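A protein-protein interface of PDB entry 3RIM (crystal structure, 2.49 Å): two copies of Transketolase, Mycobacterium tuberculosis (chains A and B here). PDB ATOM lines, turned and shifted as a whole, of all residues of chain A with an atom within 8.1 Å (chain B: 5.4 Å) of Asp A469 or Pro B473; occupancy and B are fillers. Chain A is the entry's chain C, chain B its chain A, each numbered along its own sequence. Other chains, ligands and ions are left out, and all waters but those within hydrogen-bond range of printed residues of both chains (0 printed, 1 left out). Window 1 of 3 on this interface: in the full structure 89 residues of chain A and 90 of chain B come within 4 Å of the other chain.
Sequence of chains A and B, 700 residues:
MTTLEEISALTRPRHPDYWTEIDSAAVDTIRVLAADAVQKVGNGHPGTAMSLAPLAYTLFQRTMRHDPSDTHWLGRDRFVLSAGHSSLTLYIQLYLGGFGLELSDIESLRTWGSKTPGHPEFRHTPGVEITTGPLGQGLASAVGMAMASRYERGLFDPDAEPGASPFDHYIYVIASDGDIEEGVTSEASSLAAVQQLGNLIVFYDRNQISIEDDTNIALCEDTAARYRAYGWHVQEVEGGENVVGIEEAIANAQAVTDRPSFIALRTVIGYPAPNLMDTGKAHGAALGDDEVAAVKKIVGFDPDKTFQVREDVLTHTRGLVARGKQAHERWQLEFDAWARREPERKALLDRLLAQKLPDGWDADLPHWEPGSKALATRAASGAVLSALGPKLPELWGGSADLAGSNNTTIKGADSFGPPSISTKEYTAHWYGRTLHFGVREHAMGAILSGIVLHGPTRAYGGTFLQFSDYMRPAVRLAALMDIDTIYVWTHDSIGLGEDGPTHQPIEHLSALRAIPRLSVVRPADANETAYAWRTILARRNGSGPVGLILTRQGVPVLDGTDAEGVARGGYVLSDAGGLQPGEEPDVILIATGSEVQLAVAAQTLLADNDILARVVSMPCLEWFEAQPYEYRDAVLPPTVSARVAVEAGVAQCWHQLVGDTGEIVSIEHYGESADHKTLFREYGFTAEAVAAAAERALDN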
ATOM      1  N   GLU A 441      27.916  18.250 -27.209  1.00  0.00           N
ATOM      2  CA  GLU A 441      27.330  19.549 -27.608  1.00  0.00           C
ATOM      3  C   GLU A 441      28.167  20.796 -27.201  1.00  0.00           C
ATOM      4  O   GLU A 441      28.317  21.718 -27.962  1.00  0.00           O
ATOM      5  CB  GLU A 441      25.925  19.675 -27.069  1.00  0.00           C
ATOM      6  CG  GLU A 441      24.963  18.539 -27.498  1.00  0.00           C
ATOM      7  CD  GLU A 441      25.061  17.286 -26.634  1.00  0.00           C
ATOM      8  OE1 GLU A 441      25.731  17.300 -25.580  1.00  0.00           O
ATOM      9  OE2 GLU A 441      24.440  16.282 -27.027  1.00  0.00           O
ATOM     10  N   HIS A 442      28.699  20.824 -25.993  1.00  0.00           N
ATOM     11  CA  HIS A 442      29.465  21.961 -25.520  1.00  0.00           C
ATOM     12  C   HIS A 442      30.710  22.213 -26.400  1.00  0.00           C
ATOM     13  O   HIS A 442      30.906  23.286 -26.965  1.00  0.00           O
ATOM     14  CB  HIS A 442      29.845  21.732 -24.065  1.00  0.00           C
ATOM     15  CG  HIS A 442      30.186  22.984 -23.327  1.00  0.00           C
ATOM     16  ND1 HIS A 442      30.433  23.002 -21.967  1.00  0.00           N
ATOM     17  CD2 HIS A 442      30.318  24.262 -23.753  1.00  0.00           C
ATOM     18  CE1 HIS A 442      30.757  24.231 -21.598  1.00  0.00           C
ATOM     19  NE2 HIS A 442      30.680  25.016 -22.657  1.00  0.00           N
ATOM     20  N   THR A 463      21.946  20.016 -32.884  1.00  0.00           N
ATOM     21  CA  THR A 463      21.474  19.126 -31.818  1.00  0.00           C
ATOM     22  C   THR A 463      19.990  19.380 -31.466  1.00  0.00           C
ATOM     23  O   THR A 463      19.357  20.236 -32.039  1.00  0.00           O
ATOM     24  CB  THR A 463      22.420  19.214 -30.600  1.00  0.00           C
ATOM     25  OG1 THR A 463      22.156  18.120 -29.732  1.00  0.00           O
ATOM     26  CG2 THR A 463      22.266  20.528 -29.829  1.00  0.00           C
ATOM     27  N   PHE A 464      19.418  18.644 -30.546  1.00  0.00           N
ATOM     28  CA  PHE A 464      18.070  19.004 -30.066  1.00  0.00           C
ATOM     29  C   PHE A 464      18.027  20.310 -29.252  1.00  0.00           C
ATOM     30  O   PHE A 464      18.838  20.510 -28.367  1.00  0.00           O
ATOM     31  CB  PHE A 464      17.419  17.867 -29.223  1.00  0.00           C
ATOM     32  CG  PHE A 464      17.241  16.562 -29.963  1.00  0.00           C
ATOM     33  CD1 PHE A 464      17.236  16.495 -31.359  1.00  0.00           C
ATOM     34  CD2 PHE A 464      17.085  15.371 -29.247  1.00  0.00           C
ATOM     35  CE1 PHE A 464      17.119  15.248 -32.016  1.00  0.00           C
ATOM     36  CE2 PHE A 464      16.909  14.155 -29.901  1.00  0.00           C
ATOM     37  CZ  PHE A 464      16.932  14.091 -31.284  1.00  0.00           C
ATOM     38  N   LEU A 465      17.073  21.177 -29.532  1.00  0.00           N
ATOM     39  CA  LEU A 465      16.914  22.392 -28.749  1.00  0.00           C
ATOM     40  C   LEU A 465      17.200  22.207 -27.233  1.00  0.00           C
ATOM     41  O   LEU A 465      18.009  22.957 -26.639  1.00  0.00           O
ATOM     42  CB  LEU A 465      15.523  22.990 -28.959  1.00  0.00           C
ATOM     43  CG  LEU A 465      15.283  24.307 -28.175  1.00  0.00           C
ATOM     44  CD1 LEU A 465      16.368  25.459 -28.476  1.00  0.00           C
ATOM     45  CD2 LEU A 465      13.878  24.774 -28.400  1.00  0.00           C
ATOM     46  N   GLN A 466      16.585  21.182 -26.636  1.00  0.00           N
ATOM     47  CA  GLN A 466      16.819  20.864 -25.258  1.00  0.00           C
ATOM     48  C   GLN A 466      18.294  21.013 -24.837  1.00  0.00           C
ATOM     49  O   GLN A 466      18.581  21.495 -23.736  1.00  0.00           O
ATOM     50  CB  GLN A 466      16.363  19.446 -25.008  1.00  0.00           C
ATOM     51  CG  GLN A 466      16.580  19.004 -23.567  1.00  0.00           C
ATOM     52  CD  GLN A 466      15.771  19.802 -22.561  1.00  0.00           C
ATOM     53  OE1 GLN A 466      14.576  20.013 -22.741  1.00  0.00           O
ATOM     54  NE2 GLN A 466      16.413  20.216 -21.476  1.00  0.00           N
ATOM     55  N   PHE A 467      19.212  20.603 -25.720  1.00  0.00           N
ATOM     56  CA  PHE A 467      20.625  20.496 -25.361  1.00  0.00           C
ATOM     57  C   PHE A 467      21.439  21.727 -25.672  1.00  0.00           C
ATOM     58  O   PHE A 467      22.658  21.749 -25.544  1.00  0.00           O
ATOM     59  CB  PHE A 467      21.271  19.232 -25.916  1.00  0.00           C
ATOM     60  CG  PHE A 467      20.507  17.984 -25.584  1.00  0.00           C
ATOM     61  CD1 PHE A 467      20.189  17.678 -24.269  1.00  0.00           C
ATOM     62  CD2 PHE A 467      20.086  17.138 -26.594  1.00  0.00           C
ATOM     63  CE1 PHE A 467      19.449  16.544 -23.963  1.00  0.00           C
ATOM     64  CE2 PHE A 467      19.344  15.991 -26.324  1.00  0.00           C
ATOM     65  CZ  PHE A 467      19.009  15.681 -25.023  1.00  0.00           C
ATOM     66  N   SER A 468      20.745  22.797 -26.030  1.00  0.00           N
ATOM     67  CA  SER A 468      21.398  24.060 -26.005  1.00  0.00           C
ATOM     68  C   SER A 468      21.793  24.300 -24.541  1.00  0.00           C
ATOM     69  O   SER A 468      22.701  25.080 -24.258  1.00  0.00           O
ATOM     70  CB  SER A 468      20.460  25.098 -26.473  1.00  0.00           C
ATOM     71  OG  SER A 468      19.310  25.021 -25.676  1.00  0.00           O
ATOM     72  N   ASP A 469      21.138  23.608 -23.620  1.00  0.00           N
ATOM     73  CA  ASP A 469      21.571  23.655 -22.247  1.00  0.00           C
ATOM     74  C   ASP A 469      23.006  23.170 -22.074  1.00  0.00           C
ATOM     75  O   ASP A 469      23.752  23.733 -21.254  1.00  0.00           O
ATOM     76  CB  ASP A 469      20.643  22.849 -21.337  1.00  0.00           C
ATOM     77  CG  ASP A 469      19.437  23.642 -20.883  1.00  0.00           C
ATOM     78  OD1 ASP A 469      19.419  24.876 -21.054  1.00  0.00           O
ATOM     79  OD2 ASP A 469      18.483  23.018 -20.366  1.00  0.00           O
ATOM     80  N   TYR A 470      23.406  22.148 -22.837  1.00  0.00           N
ATOM     81  CA  TYR A 470      24.753  21.605 -22.675  1.00  0.00           C
ATOM     82  C   TYR A 470      25.866  22.541 -23.209  1.00  0.00           C
ATOM     83  O   TYR A 470      27.014  22.495 -22.737  1.00  0.00           O
ATOM     84  CB  TYR A 470      24.867  20.224 -23.288  1.00  0.00           C
ATOM     85  CG  TYR A 470      24.380  19.053 -22.424  1.00  0.00           C
ATOM     86  CD1 TYR A 470      25.298  18.128 -21.907  1.00  0.00           C
ATOM     87  CD2 TYR A 470      23.011  18.815 -22.220  1.00  0.00           C
ATOM     88  CE1 TYR A 470      24.895  17.015 -21.150  1.00  0.00           C
ATOM     89  CE2 TYR A 470      22.573  17.686 -21.456  1.00  0.00           C
ATOM     90  CZ  TYR A 470      23.540  16.791 -20.926  1.00  0.00           C
ATOM     91  OH  TYR A 470      23.194  15.706 -20.139  1.00  0.00           O
ATOM     92  N   MET A 471      25.498  23.408 -24.143  1.00  0.00           N
ATOM     93  CA  MET A 471      26.448  24.251 -24.847  1.00  0.00           C
ATOM     94  C   MET A 471      26.296  25.750 -24.567  1.00  0.00           C
ATOM     95  O   MET A 471      26.825  26.619 -25.267  1.00  0.00           O
ATOM     96  CB  MET A 471      26.315  23.984 -26.352  1.00  0.00           C
ATOM     97  CG  MET A 471      24.891  24.075 -26.884  1.00  0.00           C
ATOM     98  SD  MET A 471      24.803  23.406 -28.551  1.00  0.00           S
ATOM     99  CE  MET A 471      25.711  24.553 -29.499  1.00  0.00           C
ATOM    100  N   ARG A 472      25.564  26.050 -23.510  1.00  0.00           N
ATOM    101  CA  ARG A 472      25.235  27.408 -23.191  1.00  0.00           C
ATOM    102  C   ARG A 472      26.429  28.303 -22.934  1.00  0.00           C
ATOM    103  O   ARG A 472      26.410  29.459 -23.319  1.00  0.00           O
ATOM    104  CB  ARG A 472      24.324  27.421 -21.984  1.00  0.00           C
ATOM    105  CG  ARG A 472      23.573  28.699 -21.881  1.00  0.00           C
ATOM    106  CD  ARG A 472      22.275  28.572 -21.107  1.00  0.00           C
ATOM    107  NE  ARG A 472      21.872  29.938 -20.872  1.00  0.00           N
ATOM    108  CZ  ARG A 472      20.850  30.527 -21.463  1.00  0.00           C
ATOM    109  NH1 ARG A 472      20.028  29.852 -22.257  1.00  0.00           N
ATOM    110  NH2 ARG A 472      20.620  31.791 -21.212  1.00  0.00           N
ATOM    111  N   PRO A 473      27.449  27.816 -22.240  1.00  0.00           N
ATOM    112  CA  PRO A 473      28.477  28.830 -22.051  1.00  0.00           C
ATOM    113  C   PRO A 473      29.187  29.191 -23.353  1.00  0.00           C
ATOM    114  O   PRO A 473      29.750  30.256 -23.449  1.00  0.00           O
ATOM    115  CB  PRO A 473      29.443  28.199 -21.061  1.00  0.00           C
ATOM    116  CG  PRO A 473      28.659  27.032 -20.458  1.00  0.00           C
ATOM    117  CD  PRO A 473      27.675  26.601 -21.443  1.00  0.00           C
ATOM    118  N   ALA A 474      29.161  28.307 -24.344  1.00  0.00           N
ATOM    119  CA  ALA A 474      29.845  28.619 -25.628  1.00  0.00           C
ATOM    120  C   ALA A 474      29.045  29.595 -26.472  1.00  0.00           C
ATOM    121  O   ALA A 474      29.596  30.574 -26.988  1.00  0.00           O
ATOM    122  CB  ALA A 474      30.192  27.378 -26.376  1.00  0.00           C
ATOM    123  N   VAL A 475      27.740  29.328 -26.547  1.00  0.00           N
ATOM    124  CA  VAL A 475      26.712  30.184 -27.175  1.00  0.00           C
ATOM    125  C   VAL A 475      26.780  31.633 -26.682  1.00  0.00           C
ATOM    126  O   VAL A 475      26.816  32.574 -27.476  1.00  0.00           O
ATOM    127  CB  VAL A 475      25.269  29.597 -26.898  1.00  0.00           C
ATOM    128  CG1 VAL A 475      24.179  30.593 -27.257  1.00  0.00           C
ATOM    129  CG2 VAL A 475      25.081  28.292 -27.639  1.00  0.00           C
ATOM    130  N   TRP A 489      18.965  24.116 -33.937  1.00  0.00           N
ATOM    131  CA  TRP A 489      18.347  23.356 -32.884  1.00  0.00           C
ATOM    132  C   TRP A 489      17.037  22.729 -33.320  1.00  0.00           C
ATOM    133  O   TRP A 489      16.054  23.431 -33.577  1.00  0.00           O
ATOM    134  CB  TRP A 489      18.179  24.200 -31.622  1.00  0.00           C
ATOM    135  CG  TRP A 489      19.463  24.403 -30.863  1.00  0.00           C
ATOM    136  CD1 TRP A 489      20.306  23.437 -30.413  1.00  0.00           C
ATOM    137  CD2 TRP A 489      20.051  25.670 -30.464  1.00  0.00           C
ATOM    138  NE1 TRP A 489      21.379  24.011 -29.751  1.00  0.00           N
ATOM    139  CE2 TRP A 489      21.238  25.378 -29.770  1.00  0.00           C
ATOM    140  CE3 TRP A 489      19.670  27.008 -30.607  1.00  0.00           C
ATOM    141  CZ2 TRP A 489      22.063  26.386 -29.248  1.00  0.00           C
ATOM    142  CZ3 TRP A 489      20.460  27.984 -30.085  1.00  0.00           C
ATOM    143  CH2 TRP A 489      21.655  27.688 -29.416  1.00  0.00           C
ATOM    144  N   THR A 502      12.191  14.960 -20.363  1.00  0.00           N
ATOM    145  CA  THR A 502      13.604  15.244 -20.247  1.00  0.00           C
ATOM    146  C   THR A 502      14.103  15.874 -21.544  1.00  0.00           C
ATOM    147  O   THR A 502      15.132  16.574 -21.515  1.00  0.00           O
ATOM    148  CB  THR A 502      14.477  13.991 -20.032  1.00  0.00           C
ATOM    149  OG1 THR A 502      14.368  13.156 -21.174  1.00  0.00           O
ATOM    150  CG2 THR A 502      14.120  13.227 -18.797  1.00  0.00           C
ATOM    151  N   PRO A 505      11.631  20.810 -24.845  1.00  0.00           N
ATOM    152  CA  PRO A 505      11.922  22.169 -24.410  1.00  0.00           C
ATOM    153  C   PRO A 505      10.674  22.883 -23.914  1.00  0.00           C
ATOM    154  O   PRO A 505       9.604  22.730 -24.479  1.00  0.00           O
ATOM    155  CB  PRO A 505      12.445  22.844 -25.680  1.00  0.00           C
ATOM    156  CG  PRO A 505      12.794  21.706 -26.622  1.00  0.00           C
ATOM    157  CD  PRO A 505      11.816  20.649 -26.301  1.00  0.00           C
ATOM    158  N   ILE A 506      10.842  23.647 -22.839  1.00  0.00           N
ATOM    159  CA  ILE A 506       9.785  24.463 -22.262  1.00  0.00           C
ATOM    160  C   ILE A 506      10.304  25.880 -22.061  1.00  0.00           C
ATOM    161  O   ILE A 506       9.759  26.825 -22.626  1.00  0.00           O
ATOM    162  CB  ILE A 506       9.287  23.915 -20.884  1.00  0.00           C
ATOM    163  CG1 ILE A 506       8.971  22.422 -20.948  1.00  0.00           C
ATOM    164  CG2 ILE A 506       8.033  24.649 -20.478  1.00  0.00           C
ATOM    165  CD1 ILE A 506       7.642  22.096 -21.689  1.00  0.00           C
ATOM    166  N   GLU A 507      11.382  26.000 -21.281  1.00  0.00           N
ATOM    167  CA  GLU A 507      11.985  27.295 -20.971  1.00  0.00           C
ATOM    168  C   GLU A 507      13.035  27.811 -21.976  1.00  0.00           C
ATOM    169  O   GLU A 507      13.525  28.950 -21.848  1.00  0.00           O
ATOM    170  CB  GLU A 507      12.592  27.269 -19.570  1.00  0.00           C
ATOM    171  CG  GLU A 507      13.872  26.432 -19.433  1.00  0.00           C
ATOM    172  CD  GLU A 507      13.685  24.917 -19.373  1.00  0.00           C
ATOM    173  OE1 GLU A 507      12.580  24.393 -19.534  1.00  0.00           O
ATOM    174  OE2 GLU A 507      14.680  24.222 -19.204  1.00  0.00           O
ATOM    175  N   HIS A 508      13.329  27.009 -22.986  1.00  0.00           N
ATOM    176  CA  HIS A 508      14.519  27.227 -23.815  1.00  0.00           C
ATOM    177  C   HIS A 508      14.464  28.459 -24.721  1.00  0.00           C
ATOM    178  O   HIS A 508      15.403  29.269 -24.737  1.00  0.00           O
ATOM    179  CB  HIS A 508      14.924  25.944 -24.552  1.00  0.00           C
ATOM    180  CG  HIS A 508      15.226  24.812 -23.638  1.00  0.00           C
ATOM    181  ND1 HIS A 508      14.242  24.135 -22.949  1.00  0.00           N
ATOM    182  CD2 HIS A 508      16.407  24.269 -23.246  1.00  0.00           C
ATOM    183  CE1 HIS A 508      14.796  23.202 -22.192  1.00  0.00           C
ATOM    184  NE2 HIS A 508      16.111  23.268 -22.344  1.00  0.00           N
ATOM    185  N   ALA A 511      14.851  31.474 -22.434  1.00  0.00           N
ATOM    186  CA  ALA A 511      16.193  31.435 -21.896  1.00  0.00           C
ATOM    187  C   ALA A 511      17.236  31.830 -22.949  1.00  0.00           C
ATOM    188  O   ALA A 511      18.218  32.492 -22.634  1.00  0.00           O
ATOM    189  CB  ALA A 511      16.472  30.077 -21.401  1.00  0.00           C
ATOM    190  N   LEU A 512      17.012  31.415 -24.202  1.00  0.00           N
ATOM    191  CA  LEU A 512      17.935  31.712 -25.269  1.00  0.00           C
ATOM    192  C   LEU A 512      17.724  33.123 -25.777  1.00  0.00           C
ATOM    193  O   LEU A 512      18.712  33.812 -26.101  1.00  0.00           O
ATOM    194  CB  LEU A 512      17.742  30.731 -26.406  1.00  0.00           C
ATOM    195  CG  LEU A 512      18.199  29.311 -26.199  1.00  0.00           C
ATOM    196  CD1 LEU A 512      17.734  28.535 -27.423  1.00  0.00           C
ATOM    197  CD2 LEU A 512      19.748  29.246 -26.011  1.00  0.00           C
ATOM    198  N   GLN B 137      23.978  12.540 -17.297  1.00  0.00           N
ATOM    199  CA  GLN B 137      23.402  12.946 -16.029  1.00  0.00           C
ATOM    200  C   GLN B 137      23.362  11.814 -15.001  1.00  0.00           C
ATOM    201  O   GLN B 137      23.742  11.998 -13.861  1.00  0.00           O
ATOM    202  CB  GLN B 137      22.009  13.569 -16.221  1.00  0.00           C
ATOM    203  CG  GLN B 137      21.983  14.897 -16.979  1.00  0.00           C
ATOM    204  CD  GLN B 137      23.045  15.910 -16.518  1.00  0.00           C
ATOM    205  OE1 GLN B 137      23.302  16.037 -15.308  1.00  0.00           O
ATOM    206  NE2 GLN B 137      23.645  16.660 -17.483  1.00  0.00           N
ATOM    207  N   HIS B 442      29.346  21.573 -13.785  1.00  0.00           N
ATOM    208  CA  HIS B 442      28.344  20.683 -14.295  1.00  0.00           C
ATOM    209  C   HIS B 442      28.267  19.400 -13.432  1.00  0.00           C
ATOM    210  O   HIS B 442      27.166  19.033 -12.965  1.00  0.00           O
ATOM    211  CB  HIS B 442      28.580  20.385 -15.776  1.00  0.00           C
ATOM    212  CG  HIS B 442      27.402  19.752 -16.451  1.00  0.00           C
ATOM    213  ND1 HIS B 442      27.389  19.470 -17.793  1.00  0.00           N
ATOM    214  CD2 HIS B 442      26.193  19.366 -15.967  1.00  0.00           C
ATOM    215  CE1 HIS B 442      26.234  18.916 -18.115  1.00  0.00           C
ATOM    216  NE2 HIS B 442      25.487  18.845 -17.022  1.00  0.00           N
ATOM    217  N   ASP B 469      25.555  28.642 -16.177  1.00  0.00           N
ATOM    218  CA  ASP B 469      25.572  28.194 -17.541  1.00  0.00           C
ATOM    219  C   ASP B 469      26.298  26.861 -17.720  1.00  0.00           C
ATOM    220  O   ASP B 469      25.900  26.060 -18.561  1.00  0.00           O
ATOM    221  CB  ASP B 469      26.193  29.245 -18.414  1.00  0.00           C
ATOM    222  CG  ASP B 469      25.214  30.341 -18.773  1.00  0.00           C
ATOM    223  OD1 ASP B 469      23.981  30.161 -18.511  1.00  0.00           O
ATOM    224  OD2 ASP B 469      25.697  31.363 -19.346  1.00  0.00           O
ATOM    225  N   TYR B 470      27.338  26.599 -16.928  1.00  0.00           N
ATOM    226  CA  TYR B 470      28.025  25.334 -17.071  1.00  0.00           C
ATOM    227  C   TYR B 470      27.242  24.147 -16.550  1.00  0.00           C
ATOM    228  O   TYR B 470      27.455  23.040 -16.994  1.00  0.00           O
ATOM    229  CB  TYR B 470      29.408  25.365 -16.432  1.00  0.00           C
ATOM    230  CG  TYR B 470      30.484  26.044 -17.290  1.00  0.00           C
ATOM    231  CD1 TYR B 470      31.534  25.307 -17.822  1.00  0.00           C
ATOM    232  CD2 TYR B 470      30.482  27.418 -17.505  1.00  0.00           C
ATOM    233  CE1 TYR B 470      32.529  25.908 -18.583  1.00  0.00           C
ATOM    234  CE2 TYR B 470      31.492  28.033 -18.272  1.00  0.00           C
ATOM    235  CZ  TYR B 470      32.496  27.261 -18.803  1.00  0.00           C
ATOM    236  OH  TYR B 470      33.483  27.825 -19.554  1.00  0.00           O
ATOM    237  N   MET B 471      26.307  24.377 -15.641  1.00  0.00           N
ATOM    238  CA  MET B 471      25.644  23.292 -14.944  1.00  0.00           C
ATOM    239  C   MET B 471      24.141  23.212 -15.221  1.00  0.00           C
ATOM    240  O   MET B 471      23.373  22.534 -14.479  1.00  0.00           O
ATOM    241  CB  MET B 471      25.893  23.448 -13.464  1.00  0.00           C
ATOM    242  CG  MET B 471      25.564  24.789 -12.953  1.00  0.00           C
ATOM    243  SD  MET B 471      26.224  25.022 -11.284  1.00  0.00           S
ATOM    244  CE  MET B 471      25.137  24.144 -10.298  1.00  0.00           C
ATOM    245  N   ARG B 472      23.729  23.907 -16.278  1.00  0.00           N
ATOM    246  CA  ARG B 472      22.325  24.089 -16.571  1.00  0.00           C
ATOM    247  C   ARG B 472      21.545  22.806 -16.727  1.00  0.00           C
ATOM    248  O   ARG B 472      20.423  22.718 -16.189  1.00  0.00           O
ATOM    249  CB  ARG B 472      22.157  24.962 -17.789  1.00  0.00           C
ATOM    250  CG  ARG B 472      20.818  25.559 -17.801  1.00  0.00           C
ATOM    251  CD  ARG B 472      20.736  26.780 -18.661  1.00  0.00           C
ATOM    252  NE  ARG B 472      19.339  27.087 -18.894  1.00  0.00           N
ATOM    253  CZ  ARG B 472      18.678  28.021 -18.229  1.00  0.00           C
ATOM    254  NH1 ARG B 472      19.312  28.758 -17.310  1.00  0.00           N
ATOM    255  NH2 ARG B 472      17.381  28.233 -18.507  1.00  0.00           N
ATOM    256  N   PRO B 473      22.120  21.800 -17.426  1.00  0.00           N
ATOM    257  CA  PRO B 473      21.292  20.618 -17.659  1.00  0.00           C
ATOM    258  C   PRO B 473      20.975  19.874 -16.358  1.00  0.00           C
ATOM    259  O   PRO B 473      19.949  19.192 -16.255  1.00  0.00           O
ATOM    260  CB  PRO B 473      22.135  19.760 -18.617  1.00  0.00           C
ATOM    261  CG  PRO B 473      23.185  20.658 -19.146  1.00  0.00           C
ATOM    262  CD  PRO B 473      23.413  21.710 -18.134  1.00  0.00           C
ATOM    263  N   ALA B 474      21.820  20.005 -15.359  1.00  0.00           N
ATOM    264  CA  ALA B 474      21.596  19.326 -14.091  1.00  0.00           C
ATOM    265  C   ALA B 474      20.534  20.054 -13.251  1.00  0.00           C
ATOM    266  O   ALA B 474      19.676  19.443 -12.572  1.00  0.00           O
ATOM    267  CB  ALA B 474      22.889  19.268 -13.330  1.00  0.00           C
ATOM    268  N   VAL B 475      20.583  21.381 -13.315  1.00  0.00           N
ATOM    269  CA  VAL B 475      19.651  22.218 -12.604  1.00  0.00           C
ATOM    270  C   VAL B 475      18.228  21.943 -13.142  1.00  0.00           C
ATOM    271  O   VAL B 475      17.238  21.832 -12.388  1.00  0.00           O
ATOM    272  CB  VAL B 475      20.037  23.654 -12.854  1.00  0.00           C
ATOM    273  CG1 VAL B 475      18.942  24.581 -12.355  1.00  0.00           C
ATOM    274  CG2 VAL B 475      21.425  23.981 -12.208  1.00  0.00           C
ATOM    275  N   ARG B 476      18.127  21.844 -14.453  1.00  0.00           N
ATOM    276  CA  ARG B 476      16.899  21.614 -15.115  1.00  0.00           C
ATOM    277  C   ARG B 476      16.295  20.304 -14.756  1.00  0.00           C
ATOM    278  O   ARG B 476      15.120  20.180 -14.552  1.00  0.00           O
ATOM    279  CB  ARG B 476      17.155  21.662 -16.577  1.00  0.00           C
ATOM    280  CG  ARG B 476      16.029  21.989 -17.334  1.00  0.00           C
ATOM    281  CD  ARG B 476      15.480  20.895 -17.989  1.00  0.00           C
ATOM    282  NE  ARG B 476      14.358  21.347 -18.721  1.00  0.00           N
ATOM    283  CZ  ARG B 476      13.565  20.567 -19.406  1.00  0.00           C
ATOM    284  NH1 ARG B 476      13.761  19.297 -19.422  1.00  0.00           N
ATOM    285  NH2 ARG B 476      12.574  21.065 -20.053  1.00  0.00           N
ATOM    286  N   LEU B 477      17.157  19.324 -14.694  1.00  0.00           N
ATOM    287  CA  LEU B 477      16.752  17.980 -14.347  1.00  0.00           C
ATOM    288  C   LEU B 477      16.294  17.924 -12.885  1.00  0.00           C
ATOM    289  O   LEU B 477      15.322  17.244 -12.572  1.00  0.00           O
ATOM    290  CB  LEU B 477      17.886  17.020 -14.626  1.00  0.00           C
ATOM    291  CG  LEU B 477      17.483  15.579 -14.846  1.00  0.00           C
ATOM    292  CD1 LEU B 477      16.699  15.373 -16.142  1.00  0.00           C
ATOM    293  CD2 LEU B 477      18.725  14.688 -14.840  1.00  0.00           C
ATOM    294  N   ALA B 478      16.968  18.672 -12.000  1.00  0.00           N
ATOM    295  CA  ALA B 478      16.557  18.717 -10.587  1.00  0.00           C
ATOM    296  C   ALA B 478      15.137  19.273 -10.495  1.00  0.00           C
ATOM    297  O   ALA B 478      14.264  18.704  -9.793  1.00  0.00           O
ATOM    298  CB  ALA B 478      17.513  19.548  -9.748  1.00  0.00           C
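His A442 touches Tyr B470 (CE1 to CE1, 3.9 Å).
O of Asp A469 touches CD of Pro B473, at 3.7 Å.
Tyr A470 touches His B442.
Tyr A470 touches Pro B473 (CE2 to CB, 3.5 Å).
Tyr B470 touches Pro A473 (CE2 to CB, 3.5 Å).
Arg B476 touches Thr A502 (NH1 to O, 3.7 Å).
Ala A511 touches Arg B472 (CB to NH2, 3.5 Å).
His A442 touches Tyr B470, and with the chains exchanged Tyr A470 touches His B442.
Asp A469 touches Pro B473, and with the chains exchanged Pro A473 touches Asp B469.
Tyr A470 touches Pro B473, and with the chains exchanged Pro A473 touches Tyr B470.
Positions printed for both chains: 442, 469, 470, 471, 472, 473, 474 and 475.
NE2 of Gln A466 sits at hydrogen-bond distance from NE2 of His A508 (3.2 Å).
OD2 of Asp A469 lies within hydrogen-bond range of NE2 of His A508 (3.1 Å).
A ring nitrogen (NE2) of His B442 sits at hydrogen-bond distance from the side-chain amide nitrogen of Gln B137.
OD1 of Asp A469 is in salt-bridge range of NE of Arg B472, 3.1 Å away.
The side-chain hydroxyl (OH) of Tyr A470 is in hydrogen-bond range of the side-chain amide nitrogen (NE2) of Gln B137 (2.9 Å).
The side-chain amide nitrogen of Gln A466 lies close to the guanidinium group of Arg B476 (3.5 Å).
OD1 of Asp B469 is in salt-bridge range of NE of Arg A472 (3.2 Å).
The guanidinium group (NE) of Arg B476 is in salt-bridge range of the side-chain carboxylate (OE2) of Glu A507, 2.9 Å away.
Asp A469 touches two residues of chain B.
Pro B473 touches just these residues of chain A: Asp A469 (3.7 Å) and Tyr A470 (3.5 Å).
No residue of chain A comes within 4 Å of Ala B474.
Of the printed residues of chain B, Ala A511 touches Arg B472.
Printed residues of chain A within 4 Å of Gln B137: Tyr A470 (2.9 Å).
Of the printed residues of chain B, Glu A507 touches Arg B476.
The nearest residue of chain A that does not touch Pro B473 is Met A471 (6.2 Å).
The nearest printed residue of chain B that does not touch Thr A502 is Leu B477 (4.3 Å).
Of the 12 printed residues of chain B, 7 touch a printed residue of chain A.
Hydrophobic or aromatic side chains of chain B that line the printed part of chain A: His B442, Tyr B470 and Pro B473.
Hydrophobic or aromatic side chains of chain A that line the printed part of chain B: His A442, Tyr A470, Pro A473, Ile A506, His A508 and Ala A511.
Among the printed residues, 16 pairs touch across the chains.
Among the printed residues, Asp or Glu carboxylates within 4 Å of a Lys or Arg side-chain nitrogen of the other chain: Asp A469 with Arg B472 (3.1 Å), Arg A472 with Asp B469 (3.2 Å) and Glu A507 with Arg B476 (2.9 Å).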
